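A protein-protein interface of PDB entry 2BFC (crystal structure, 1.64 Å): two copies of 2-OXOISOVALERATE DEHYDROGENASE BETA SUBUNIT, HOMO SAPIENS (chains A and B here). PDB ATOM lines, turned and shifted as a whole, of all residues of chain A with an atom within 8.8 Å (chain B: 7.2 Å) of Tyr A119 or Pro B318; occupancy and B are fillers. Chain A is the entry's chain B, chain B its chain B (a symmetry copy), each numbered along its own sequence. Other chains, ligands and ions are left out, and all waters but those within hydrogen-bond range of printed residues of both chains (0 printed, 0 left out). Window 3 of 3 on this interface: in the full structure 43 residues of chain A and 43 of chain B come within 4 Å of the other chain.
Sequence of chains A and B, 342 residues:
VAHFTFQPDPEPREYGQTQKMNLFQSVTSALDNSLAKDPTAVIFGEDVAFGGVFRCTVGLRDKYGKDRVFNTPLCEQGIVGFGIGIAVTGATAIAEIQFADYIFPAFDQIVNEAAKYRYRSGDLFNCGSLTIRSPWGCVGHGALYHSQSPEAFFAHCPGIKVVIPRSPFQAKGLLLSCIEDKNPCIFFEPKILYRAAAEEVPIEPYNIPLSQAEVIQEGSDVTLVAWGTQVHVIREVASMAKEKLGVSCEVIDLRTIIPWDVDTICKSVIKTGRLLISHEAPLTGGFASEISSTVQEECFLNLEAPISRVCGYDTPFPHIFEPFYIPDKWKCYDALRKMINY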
ATOM      1  N   GLU A 113     -14.291  22.239  16.981  1.00  0.00           N
ATOM      2  CA  GLU A 113     -14.449  20.800  16.711  1.00  0.00           C
ATOM      3  C   GLU A 113     -13.080  20.143  16.529  1.00  0.00           C
ATOM      4  O   GLU A 113     -12.666  19.320  17.373  1.00  0.00           O
ATOM      5  CB  GLU A 113     -15.312  20.604  15.451  1.00  0.00           C
ATOM      6  CG  GLU A 113     -16.748  21.138  15.662  1.00  0.00           C
ATOM      7  CD  GLU A 113     -17.545  20.239  16.592  1.00  0.00           C
ATOM      8  OE1 GLU A 113     -17.588  19.018  16.301  1.00  0.00           O
ATOM      9  OE2 GLU A 113     -18.049  20.688  17.653  1.00  0.00           O
ATOM     10  N   ALA A 114     -12.346  20.438  15.460  1.00  0.00           N
ATOM     11  CA  ALA A 114     -11.138  19.590  15.187  1.00  0.00           C
ATOM     12  C   ALA A 114     -10.167  19.608  16.393  1.00  0.00           C
ATOM     13  O   ALA A 114      -9.589  18.566  16.779  1.00  0.00           O
ATOM     14  CB  ALA A 114     -10.416  20.110  13.880  1.00  0.00           C
ATOM     15  N   ALA A 115      -9.885  20.814  16.919  1.00  0.00           N
ATOM     16  CA  ALA A 115      -8.843  20.902  17.968  1.00  0.00           C
ATOM     17  C   ALA A 115      -9.225  20.170  19.228  1.00  0.00           C
ATOM     18  O   ALA A 115      -8.369  19.740  19.982  1.00  0.00           O
ATOM     19  CB  ALA A 115      -8.663  22.414  18.303  1.00  0.00           C
ATOM     20  N   LYS A 116     -10.555  20.109  19.508  1.00  0.00           N
ATOM     21  CA  LYS A 116     -11.076  19.579  20.787  1.00  0.00           C
ATOM     22  C   LYS A 116     -11.599  18.145  20.686  1.00  0.00           C
ATOM     23  O   LYS A 116     -12.018  17.566  21.710  1.00  0.00           O
ATOM     24  CB  LYS A 116     -12.209  20.533  21.286  1.00  0.00           C
ATOM     25  CG  LYS A 116     -11.637  21.927  21.675  1.00  0.00           C
ATOM     26  CD  LYS A 116     -12.822  22.929  21.820  1.00  0.00           C
ATOM     27  CE  LYS A 116     -12.381  24.318  22.346  1.00  0.00           C
ATOM     28  NZ  LYS A 116     -11.223  24.939  21.524  1.00  0.00           N
ATOM     29  N   TYR A 117     -11.535  17.578  19.468  1.00  0.00           N
ATOM     30  CA  TYR A 117     -12.148  16.285  19.178  1.00  0.00           C
ATOM     31  C   TYR A 117     -11.647  15.200  20.103  1.00  0.00           C
ATOM     32  O   TYR A 117     -12.417  14.392  20.634  1.00  0.00           O
ATOM     33  CB  TYR A 117     -11.876  15.885  17.678  1.00  0.00           C
ATOM     34  CG  TYR A 117     -13.121  15.452  16.990  1.00  0.00           C
ATOM     35  CD1 TYR A 117     -13.963  16.383  16.348  1.00  0.00           C
ATOM     36  CD2 TYR A 117     -13.537  14.124  17.053  1.00  0.00           C
ATOM     37  CE1 TYR A 117     -15.137  15.941  15.717  1.00  0.00           C
ATOM     38  CE2 TYR A 117     -14.736  13.662  16.461  1.00  0.00           C
ATOM     39  CZ  TYR A 117     -15.543  14.600  15.797  1.00  0.00           C
ATOM     40  OH  TYR A 117     -16.768  14.219  15.195  1.00  0.00           O
ATOM     41  N   ARG A 118     -10.330  15.105  20.199  1.00  0.00           N
ATOM     42  CA  ARG A 118      -9.738  14.019  21.002  1.00  0.00           C
ATOM     43  C   ARG A 118      -9.919  14.241  22.508  1.00  0.00           C
ATOM     44  O   ARG A 118     -10.344  13.319  23.248  1.00  0.00           O
ATOM     45  CB  ARG A 118      -8.242  13.899  20.671  1.00  0.00           C
ATOM     46  CG  ARG A 118      -7.656  12.623  21.278  1.00  0.00           C
ATOM     47  CD  ARG A 118      -6.098  12.517  21.105  1.00  0.00           C
ATOM     48  NE  ARG A 118      -5.692  12.534  19.706  1.00  0.00           N
ATOM     49  CZ  ARG A 118      -5.581  11.416  18.933  1.00  0.00           C
ATOM     50  NH1 ARG A 118      -5.893  10.212  19.376  1.00  0.00           N
ATOM     51  NH2 ARG A 118      -5.130  11.496  17.680  1.00  0.00           N
ATOM     52  N   TYR A 119      -9.683  15.469  22.955  1.00  0.00           N
ATOM     53  CA  TYR A 119      -9.808  15.726  24.375  1.00  0.00           C
ATOM     54  C   TYR A 119     -11.236  15.412  24.843  1.00  0.00           C
ATOM     55  O   TYR A 119     -11.436  14.760  25.898  1.00  0.00           O
ATOM     56  CB  TYR A 119      -9.555  17.237  24.601  1.00  0.00           C
ATOM     57  CG  TYR A 119      -9.457  17.639  26.047  1.00  0.00           C
ATOM     58  CD1 TYR A 119      -8.305  17.352  26.757  1.00  0.00           C
ATOM     59  CD2 TYR A 119     -10.488  18.397  26.644  1.00  0.00           C
ATOM     60  CE1 TYR A 119      -8.195  17.774  28.098  1.00  0.00           C
ATOM     61  CE2 TYR A 119     -10.377  18.872  27.973  1.00  0.00           C
ATOM     62  CZ  TYR A 119      -9.209  18.543  28.666  1.00  0.00           C
ATOM     63  OH  TYR A 119      -9.124  19.007  29.970  1.00  0.00           O
ATOM     64  N   ARG A 120     -12.202  16.016  24.123  1.00  0.00           N
ATOM     65  CA  ARG A 120     -13.556  16.045  24.650  1.00  0.00           C
ATOM     66  C   ARG A 120     -14.158  14.618  24.661  1.00  0.00           C
ATOM     67  O   ARG A 120     -15.232  14.358  25.317  1.00  0.00           O
ATOM     68  CB  ARG A 120     -14.433  17.038  23.849  1.00  0.00           C
ATOM     69  CG  ARG A 120     -14.877  16.439  22.504  1.00  0.00           C
ATOM     70  CD  ARG A 120     -15.440  17.553  21.638  1.00  0.00           C
ATOM     71  NE  ARG A 120     -15.873  16.969  20.380  1.00  0.00           N
ATOM     72  CZ  ARG A 120     -16.389  17.705  19.345  1.00  0.00           C
ATOM     73  NH1 ARG A 120     -16.354  19.041  19.431  1.00  0.00           N
ATOM     74  NH2 ARG A 120     -16.859  17.119  18.234  1.00  0.00           N
ATOM     75  N   SER A 121     -13.553  13.703  23.920  1.00  0.00           N
ATOM     76  CA  SER A 121     -14.127  12.345  23.839  1.00  0.00           C
ATOM     77  C   SER A 121     -13.361  11.409  24.740  1.00  0.00           C
ATOM     78  O   SER A 121     -13.660  10.236  24.758  1.00  0.00           O
ATOM     79  CB  SER A 121     -14.049  11.826  22.382  1.00  0.00           C
ATOM     80  OG  SER A 121     -12.672  11.595  22.022  1.00  0.00           O
ATOM     81  N   GLY A 122     -12.360  11.878  25.470  1.00  0.00           N
ATOM     82  CA  GLY A 122     -11.545  10.912  26.259  1.00  0.00           C
ATOM     83  C   GLY A 122     -10.690  10.017  25.366  1.00  0.00           C
ATOM     84  O   GLY A 122     -10.331   8.922  25.811  1.00  0.00           O
ATOM     85  N   ASP A 123     -10.370  10.486  24.156  1.00  0.00           N
ATOM     86  CA  ASP A 123      -9.646   9.678  23.158  1.00  0.00           C
ATOM     87  C   ASP A 123     -10.521   8.521  22.631  1.00  0.00           C
ATOM     88  O   ASP A 123     -10.002   7.593  22.062  1.00  0.00           O
ATOM     89  CB  ASP A 123      -8.294   9.140  23.677  1.00  0.00           C
ATOM     90  CG  ASP A 123      -7.403   8.693  22.517  1.00  0.00           C
ATOM     91  OD1 ASP A 123      -7.456   9.388  21.462  1.00  0.00           O
ATOM     92  OD2 ASP A 123      -6.682   7.637  22.625  1.00  0.00           O
ATOM     93  N   LEU A 124     -11.852   8.576  22.769  1.00  0.00           N
ATOM     94  CA  LEU A 124     -12.682   7.591  22.091  1.00  0.00           C
ATOM     95  C   LEU A 124     -12.755   7.914  20.596  1.00  0.00           C
ATOM     96  O   LEU A 124     -12.943   6.959  19.790  1.00  0.00           O
ATOM     97  CB  LEU A 124     -14.142   7.568  22.607  1.00  0.00           C
ATOM     98  CG  LEU A 124     -14.326   6.954  24.000  1.00  0.00           C
ATOM     99  CD1 LEU A 124     -15.815   6.923  24.384  1.00  0.00           C
ATOM    100  CD2 LEU A 124     -13.676   5.619  24.184  1.00  0.00           C
ATOM    101  N   PHE A 125     -12.671   9.203  20.198  1.00  0.00           N
ATOM    102  CA  PHE A 125     -12.704   9.563  18.769  1.00  0.00           C
ATOM    103  C   PHE A 125     -11.653  10.624  18.551  1.00  0.00           C
ATOM    104  O   PHE A 125     -11.238  11.333  19.523  1.00  0.00           O
ATOM    105  CB  PHE A 125     -14.097  10.161  18.406  1.00  0.00           C
ATOM    106  CG  PHE A 125     -15.175   9.152  18.527  1.00  0.00           C
ATOM    107  CD1 PHE A 125     -15.416   8.279  17.474  1.00  0.00           C
ATOM    108  CD2 PHE A 125     -15.921   9.061  19.698  1.00  0.00           C
ATOM    109  CE1 PHE A 125     -16.476   7.326  17.561  1.00  0.00           C
ATOM    110  CE2 PHE A 125     -16.932   8.101  19.833  1.00  0.00           C
ATOM    111  CZ  PHE A 125     -17.169   7.199  18.763  1.00  0.00           C
ATOM    112  N   ASN A 126     -11.245  10.791  17.284  1.00  0.00           N
ATOM    113  CA  ASN A 126     -10.220  11.830  17.022  1.00  0.00           C
ATOM    114  C   ASN A 126     -10.301  12.184  15.560  1.00  0.00           C
ATOM    115  O   ASN A 126     -10.932  11.458  14.802  1.00  0.00           O
ATOM    116  CB  ASN A 126      -8.810  11.290  17.413  1.00  0.00           C
ATOM    117  CG  ASN A 126      -8.288  10.248  16.452  1.00  0.00           C
ATOM    118  OD1 ASN A 126      -7.773  10.587  15.361  1.00  0.00           O
ATOM    119  ND2 ASN A 126      -8.337   8.965  16.869  1.00  0.00           N
ATOM    120  N   CYS A 127      -9.603  13.249  15.164  1.00  0.00           N
ATOM    121  CA  CYS A 127      -9.408  13.594  13.753  1.00  0.00           C
ATOM    122  C   CYS A 127      -7.969  13.884  13.489  1.00  0.00           C
ATOM    123  O   CYS A 127      -7.664  14.767  12.699  1.00  0.00           O
ATOM    124  CB  CYS A 127     -10.353  14.754  13.386  1.00  0.00           C
ATOM    125  SG  CYS A 127     -10.052  16.291  14.338  1.00  0.00           S
ATOM    126  N   PRO A 158      -5.426  25.404  21.724  1.00  0.00           N
ATOM    127  CA  PRO A 158      -4.881  24.100  22.023  1.00  0.00           C
ATOM    128  C   PRO A 158      -5.569  22.960  21.267  1.00  0.00           C
ATOM    129  O   PRO A 158      -6.806  22.875  21.180  1.00  0.00           O
ATOM    130  CB  PRO A 158      -5.171  23.916  23.518  1.00  0.00           C
ATOM    131  CG  PRO A 158      -5.126  25.431  24.038  1.00  0.00           C
ATOM    132  CD  PRO A 158      -5.771  26.192  22.918  1.00  0.00           C
ATOM    133  N   GLY A 159      -4.726  22.062  20.748  1.00  0.00           N
ATOM    134  CA  GLY A 159      -5.217  20.857  20.061  1.00  0.00           C
ATOM    135  C   GLY A 159      -5.045  20.849  18.546  1.00  0.00           C
ATOM    136  O   GLY A 159      -5.211  19.812  17.915  1.00  0.00           O
ATOM    137  N   ASN A 183      -2.426  14.369  14.805  1.00  0.00           N
ATOM    138  CA  ASN A 183      -3.191  15.504  15.331  1.00  0.00           C
ATOM    139  C   ASN A 183      -3.644  16.315  14.143  1.00  0.00           C
ATOM    140  O   ASN A 183      -2.951  16.311  13.134  1.00  0.00           O
ATOM    141  CB  ASN A 183      -2.275  16.404  16.188  1.00  0.00           C
ATOM    142  CG  ASN A 183      -1.711  15.634  17.379  1.00  0.00           C
ATOM    143  OD1 ASN A 183      -2.434  15.448  18.318  1.00  0.00           O
ATOM    144  ND2 ASN A 183      -0.470  15.143  17.308  1.00  0.00           N
ATOM    145  N   PRO A 184      -4.728  17.046  14.226  1.00  0.00           N
ATOM    146  CA  PRO A 184      -5.134  17.873  13.077  1.00  0.00           C
ATOM    147  C   PRO A 184      -4.127  19.006  12.877  1.00  0.00           C
ATOM    148  O   PRO A 184      -3.779  19.680  13.860  1.00  0.00           O
ATOM    149  CB  PRO A 184      -6.525  18.417  13.502  1.00  0.00           C
ATOM    150  CG  PRO A 184      -6.517  18.330  15.067  1.00  0.00           C
ATOM    151  CD  PRO A 184      -5.691  17.047  15.334  1.00  0.00           C
ATOM    152  N   GLY B 140     -18.218  27.792  36.518  1.00  0.00           N
ATOM    153  CA  GLY B 140     -18.188  26.707  37.510  1.00  0.00           C
ATOM    154  C   GLY B 140     -18.352  25.287  36.984  1.00  0.00           C
ATOM    155  O   GLY B 140     -17.763  24.332  37.535  1.00  0.00           O
ATOM    156  N   HIS B 141     -19.135  25.149  35.917  1.00  0.00           N
ATOM    157  CA  HIS B 141     -19.527  23.858  35.372  1.00  0.00           C
ATOM    158  C   HIS B 141     -19.816  23.908  33.890  1.00  0.00           C
ATOM    159  O   HIS B 141     -20.437  22.959  33.361  1.00  0.00           O
ATOM    160  CB  HIS B 141     -20.824  23.418  36.084  1.00  0.00           C
ATOM    161  CG  HIS B 141     -21.810  24.537  36.214  1.00  0.00           C
ATOM    162  ND1 HIS B 141     -22.004  25.223  37.402  1.00  0.00           N
ATOM    163  CD2 HIS B 141     -22.593  25.141  35.298  1.00  0.00           C
ATOM    164  CE1 HIS B 141     -22.893  26.181  37.203  1.00  0.00           C
ATOM    165  NE2 HIS B 141     -23.284  26.134  35.939  1.00  0.00           N
ATOM    166  N   GLY B 142     -19.368  24.957  33.198  1.00  0.00           N
ATOM    167  CA  GLY B 142     -19.727  25.134  31.771  1.00  0.00           C
ATOM    168  C   GLY B 142     -18.907  24.259  30.822  1.00  0.00           C
ATOM    169  O   GLY B 142     -19.227  24.176  29.668  1.00  0.00           O
ATOM    170  N   ALA B 143     -17.788  23.727  31.285  1.00  0.00           N
ATOM    171  CA  ALA B 143     -16.986  22.862  30.405  1.00  0.00           C
ATOM    172  C   ALA B 143     -16.592  23.538  29.136  1.00  0.00           C
ATOM    173  O   ALA B 143     -16.352  24.772  29.117  1.00  0.00           O
ATOM    174  CB  ALA B 143     -17.682  21.497  30.204  1.00  0.00           C
ATOM    175  N   LEU B 144     -16.442  22.773  28.038  1.00  0.00           N
ATOM    176  CA  LEU B 144     -15.747  23.311  26.904  1.00  0.00           C
ATOM    177  C   LEU B 144     -16.432  24.393  26.159  1.00  0.00           C
ATOM    178  O   LEU B 144     -15.762  25.193  25.544  1.00  0.00           O
ATOM    179  CB  LEU B 144     -15.440  22.206  25.860  1.00  0.00           C
ATOM    180  CG  LEU B 144     -14.259  21.293  26.151  1.00  0.00           C
ATOM    181  CD1 LEU B 144     -14.505  20.285  27.305  1.00  0.00           C
ATOM    182  CD2 LEU B 144     -13.945  20.489  24.861  1.00  0.00           C
ATOM    183  N   SER B 147     -17.959  28.102  28.674  1.00  0.00           N
ATOM    184  CA  SER B 147     -16.976  28.759  29.553  1.00  0.00           C
ATOM    185  C   SER B 147     -15.972  29.635  28.836  1.00  0.00           C
ATOM    186  O   SER B 147     -15.150  30.244  29.520  1.00  0.00           O
ATOM    187  CB  SER B 147     -16.100  27.674  30.172  1.00  0.00           C
ATOM    188  OG  SER B 147     -16.887  26.693  30.850  1.00  0.00           O
ATOM    189  N   THR B 315      -5.287  23.949  27.408  1.00  0.00           N
ATOM    190  CA  THR B 315      -6.197  22.833  27.175  1.00  0.00           C
ATOM    191  C   THR B 315      -7.552  23.437  26.845  1.00  0.00           C
ATOM    192  O   THR B 315      -7.762  24.647  27.065  1.00  0.00           O
ATOM    193  CB  THR B 315      -6.345  21.918  28.434  1.00  0.00           C
ATOM    194  OG1 THR B 315      -7.027  22.662  29.455  1.00  0.00           O
ATOM    195  CG2 THR B 315      -4.984  21.594  29.032  1.00  0.00           C
ATOM    196  N   PRO B 316      -8.480  22.630  26.351  1.00  0.00           N
ATOM    197  CA  PRO B 316      -9.874  23.052  26.333  1.00  0.00           C
ATOM    198  C   PRO B 316     -10.387  23.178  27.743  1.00  0.00           C
ATOM    199  O   PRO B 316      -9.729  22.733  28.711  1.00  0.00           O
ATOM    200  CB  PRO B 316     -10.573  21.908  25.607  1.00  0.00           C
ATOM    201  CG  PRO B 316      -9.438  21.209  24.786  1.00  0.00           C
ATOM    202  CD  PRO B 316      -8.297  21.283  25.753  1.00  0.00           C
ATOM    203  N   PHE B 317     -11.547  23.831  27.919  1.00  0.00           N
ATOM    204  CA  PHE B 317     -11.928  24.203  29.303  1.00  0.00           C
ATOM    205  C   PHE B 317     -12.721  23.006  29.882  1.00  0.00           C
ATOM    206  O   PHE B 317     -13.789  22.643  29.356  1.00  0.00           O
ATOM    207  CB  PHE B 317     -12.828  25.473  29.262  1.00  0.00           C
ATOM    208  CG  PHE B 317     -12.929  26.115  30.599  1.00  0.00           C
ATOM    209  CD1 PHE B 317     -13.674  25.484  31.555  1.00  0.00           C
ATOM    210  CD2 PHE B 317     -12.258  27.297  30.894  1.00  0.00           C
ATOM    211  CE1 PHE B 317     -13.748  25.989  32.840  1.00  0.00           C
ATOM    212  CE2 PHE B 317     -12.395  27.846  32.177  1.00  0.00           C
ATOM    213  CZ  PHE B 317     -13.137  27.185  33.128  1.00  0.00           C
ATOM    214  N   PRO B 318     -12.203  22.349  30.934  1.00  0.00           N
ATOM    215  CA  PRO B 318     -12.823  21.100  31.381  1.00  0.00           C
ATOM    216  C   PRO B 318     -14.049  21.243  32.277  1.00  0.00           C
ATOM    217  O   PRO B 318     -14.195  22.271  33.004  1.00  0.00           O
ATOM    218  CB  PRO B 318     -11.697  20.389  32.185  1.00  0.00           C
ATOM    219  CG  PRO B 318     -10.959  21.544  32.772  1.00  0.00           C
ATOM    220  CD  PRO B 318     -10.976  22.709  31.691  1.00  0.00           C
ATOM    221  N   HIS B 319     -14.933  20.231  32.232  1.00  0.00           N
ATOM    222  CA  HIS B 319     -16.033  20.139  33.176  1.00  0.00           C
ATOM    223  C   HIS B 319     -15.569  19.861  34.607  1.00  0.00           C
ATOM    224  O   HIS B 319     -15.536  20.768  35.462  1.00  0.00           O
ATOM    225  CB  HIS B 319     -17.011  19.050  32.694  1.00  0.00           C
ATOM    226  CG  HIS B 319     -18.206  18.867  33.586  1.00  0.00           C
ATOM    227  ND1 HIS B 319     -18.663  17.617  33.961  1.00  0.00           N
ATOM    228  CD2 HIS B 319     -19.010  19.762  34.203  1.00  0.00           C
ATOM    229  CE1 HIS B 319     -19.708  17.754  34.762  1.00  0.00           C
ATOM    230  NE2 HIS B 319     -19.943  19.040  34.927  1.00  0.00           N
ATOM    231  N   ILE B 320     -15.267  18.596  34.929  1.00  0.00           N
ATOM    232  CA  ILE B 320     -15.123  18.281  36.346  1.00  0.00           C
ATOM    233  C   ILE B 320     -13.847  18.871  36.955  1.00  0.00           C
ATOM    234  O   ILE B 320     -13.780  19.052  38.226  1.00  0.00           O
ATOM    235  CB  ILE B 320     -15.258  16.731  36.535  1.00  0.00           C
ATOM    236  CG1 ILE B 320     -15.730  16.336  37.963  1.00  0.00           C
ATOM    237  CG2 ILE B 320     -13.910  15.968  36.239  1.00  0.00           C
ATOM    238  CD1 ILE B 320     -17.209  16.803  38.184  1.00  0.00           C
ATOM    239  N   PHE B 321     -12.861  19.181  36.090  1.00  0.00           N
ATOM    240  CA  PHE B 321     -11.590  19.741  36.593  1.00  0.00           C
ATOM    241  C   PHE B 321     -11.556  21.230  36.695  1.00  0.00           C
ATOM    242  O   PHE B 321     -10.473  21.767  36.996  1.00  0.00           O
ATOM    243  CB  PHE B 321     -10.395  19.239  35.762  1.00  0.00           C
ATOM    244  CG  PHE B 321     -10.418  17.741  35.514  1.00  0.00           C
ATOM    245  CD1 PHE B 321     -10.198  16.864  36.575  1.00  0.00           C
ATOM    246  CD2 PHE B 321     -10.678  17.214  34.224  1.00  0.00           C
ATOM    247  CE1 PHE B 321     -10.245  15.483  36.375  1.00  0.00           C
ATOM    248  CE2 PHE B 321     -10.696  15.826  34.015  1.00  0.00           C
ATOM    249  CZ  PHE B 321     -10.442  14.964  35.104  1.00  0.00           C
ATOM    250  N   GLU B 322     -12.683  21.930  36.536  1.00  0.00           N
ATOM    251  CA  GLU B 322     -12.579  23.401  36.548  1.00  0.00           C
ATOM    252  C   GLU B 322     -11.838  23.956  37.765  1.00  0.00           C
ATOM    253  O   GLU B 322     -11.040  24.934  37.571  1.00  0.00           O
ATOM    254  CB  GLU B 322     -13.958  24.064  36.414  1.00  0.00           C
ATOM    255  CG  GLU B 322     -13.888  25.581  36.409  1.00  0.00           C
ATOM    256  CD  GLU B 322     -15.151  26.252  35.976  1.00  0.00           C
ATOM    257  OE1 GLU B 322     -16.007  25.603  35.315  1.00  0.00           O
ATOM    258  OE2 GLU B 322     -15.286  27.441  36.337  1.00  0.00           O
ATOM    259  N   PRO B 323     -12.090  23.459  38.994  1.00  0.00           N
ATOM    260  CA  PRO B 323     -11.399  24.024  40.160  1.00  0.00           C
ATOM    261  C   PRO B 323      -9.859  23.985  40.027  1.00  0.00           C
ATOM    262  O   PRO B 323      -9.179  24.808  40.664  1.00  0.00           O
ATOM    263  CB  PRO B 323     -11.841  23.096  41.312  1.00  0.00           C
ATOM    264  CG  PRO B 323     -13.094  22.514  40.874  1.00  0.00           C
ATOM    265  CD  PRO B 323     -13.031  22.385  39.378  1.00  0.00           C
ATOM    266  N   PHE B 324      -9.330  23.045  39.235  1.00  0.00           N
ATOM    267  CA  PHE B 324      -7.878  22.916  39.116  1.00  0.00           C
ATOM    268  C   PHE B 324      -7.370  23.655  37.898  1.00  0.00           C
ATOM    269  O   PHE B 324      -6.143  23.804  37.773  1.00  0.00           O
ATOM    270  CB  PHE B 324      -7.502  21.429  38.968  1.00  0.00           C
ATOM    271  CG  PHE B 324      -7.914  20.599  40.140  1.00  0.00           C
ATOM    272  CD1 PHE B 324      -7.162  20.687  41.321  1.00  0.00           C
ATOM    273  CD2 PHE B 324      -9.056  19.795  40.094  1.00  0.00           C
ATOM    274  CE1 PHE B 324      -7.552  19.933  42.465  1.00  0.00           C
ATOM    275  CE2 PHE B 324      -9.473  19.043  41.234  1.00  0.00           C
ATOM    276  CZ  PHE B 324      -8.708  19.109  42.426  1.00  0.00           C
ATOM    277  N   TYR B 325      -8.276  24.105  37.006  1.00  0.00           N
ATOM    278  CA  TYR B 325      -7.867  24.732  35.748  1.00  0.00           C
ATOM    279  C   TYR B 325      -7.681  26.260  35.875  1.00  0.00           C
ATOM    280  O   TYR B 325      -6.735  26.855  35.284  1.00  0.00           O
ATOM    281  CB  TYR B 325      -8.976  24.457  34.690  1.00  0.00           C
ATOM    282  CG  TYR B 325      -8.634  25.179  33.383  1.00  0.00           C
ATOM    283  CD1 TYR B 325      -7.780  24.611  32.454  1.00  0.00           C
ATOM    284  CD2 TYR B 325      -9.171  26.414  33.115  1.00  0.00           C
ATOM    285  CE1 TYR B 325      -7.430  25.301  31.284  1.00  0.00           C
ATOM    286  CE2 TYR B 325      -8.812  27.153  31.973  1.00  0.00           C
ATOM    287  CZ  TYR B 325      -7.946  26.566  31.074  1.00  0.00           C
ATOM    288  OH  TYR B 325      -7.513  27.244  29.965  1.00  0.00           O
ATOM    289  N   ILE B 326      -8.602  26.909  36.602  1.00  0.00           N
ATOM    290  CA  ILE B 326      -8.662  28.363  36.643  1.00  0.00           C
ATOM    291  C   ILE B 326      -7.470  29.021  37.371  1.00  0.00           C
ATOM    292  O   ILE B 326      -6.936  28.465  38.343  1.00  0.00           O
ATOM    293  CB  ILE B 326      -9.988  28.798  37.280  1.00  0.00           C
ATOM    294  CG1 ILE B 326     -10.115  28.184  38.662  1.00  0.00           C
ATOM    295  CG2 ILE B 326     -11.152  28.518  36.255  1.00  0.00           C
ATOM    296  CD1 ILE B 326     -11.251  28.897  39.478  1.00  0.00           C
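No position is printed for both chains. Of the 6 pairs that touch across the chains among the printed residues, none has its exchanged pair printed and touching as well.
Of the printed residues of chain B, Lys A116 touches Leu B144 (3.97 Å) and Pro B316 (3.9 Å). Tyr A119 touches just these residues of chain B: Pro B316 (3.5 Å) and Pro B318 (3.7 Å). Of the printed residues of chain A, Leu B144 touches Lys A116 and Arg A120. Of the printed residues of chain A, Thr B315 touches Pro A158 (3.7 Å). Pro B316 touches just these residues of chain A: Lys A116 (3.9 Å) and Tyr A119 (3.5 Å). Pro B318 touches one residue of chain A. The nearest residue of chain B that does not touch Tyr A119 is Thr B315 (4.2 Å). The nearest residue of chain A that does not touch Pro B318 is Arg A120 (8.4 Å). The nearest printed residue of chain B that does not touch Lys A116 is Phe B317 (5.7 Å).
Of the 19 printed residues of chain A, 4 touch a printed residue of chain B. Printed residues of chain A that touch a printed residue of chain B: Lys A116, Tyr A119, Arg A120 and Pro A158. Hydrophobic or aromatic side chains of chain A within 4 Å of the printed part of chain B: Tyr A119 and Pro A158. Printed residues of chain B that touch a printed residue of chain A: Leu B144, Thr B315, Pro B316 and Pro B318. Hydrophobic or aromatic side chains of chain B that line the printed part of chain A: Leu B144, Pro B316 and Pro B318. Among the printed residues, no Asp or Glu carboxylate lies within 4 Å of a Lys or Arg side-chain nitrogen of the other chain.
Among the printed residues, pairs that only touch across the chains: Tyr A119 with Pro B316, Arg A120 with Leu B144, Tyr A119 with Pro B318, Pro A158 with Thr B315, Lys A116 with Pro B316 and Lys A116 with Leu B144.
The backbone carbonyl oxygen (O) of Phe B317 sits at hydrogen-bond distance from the backbone NH (N) of Leu B144 (3.0 Å). OE1 of Glu A113 lies within salt-bridge range of NH2 of Arg A120 (2.8 Å).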
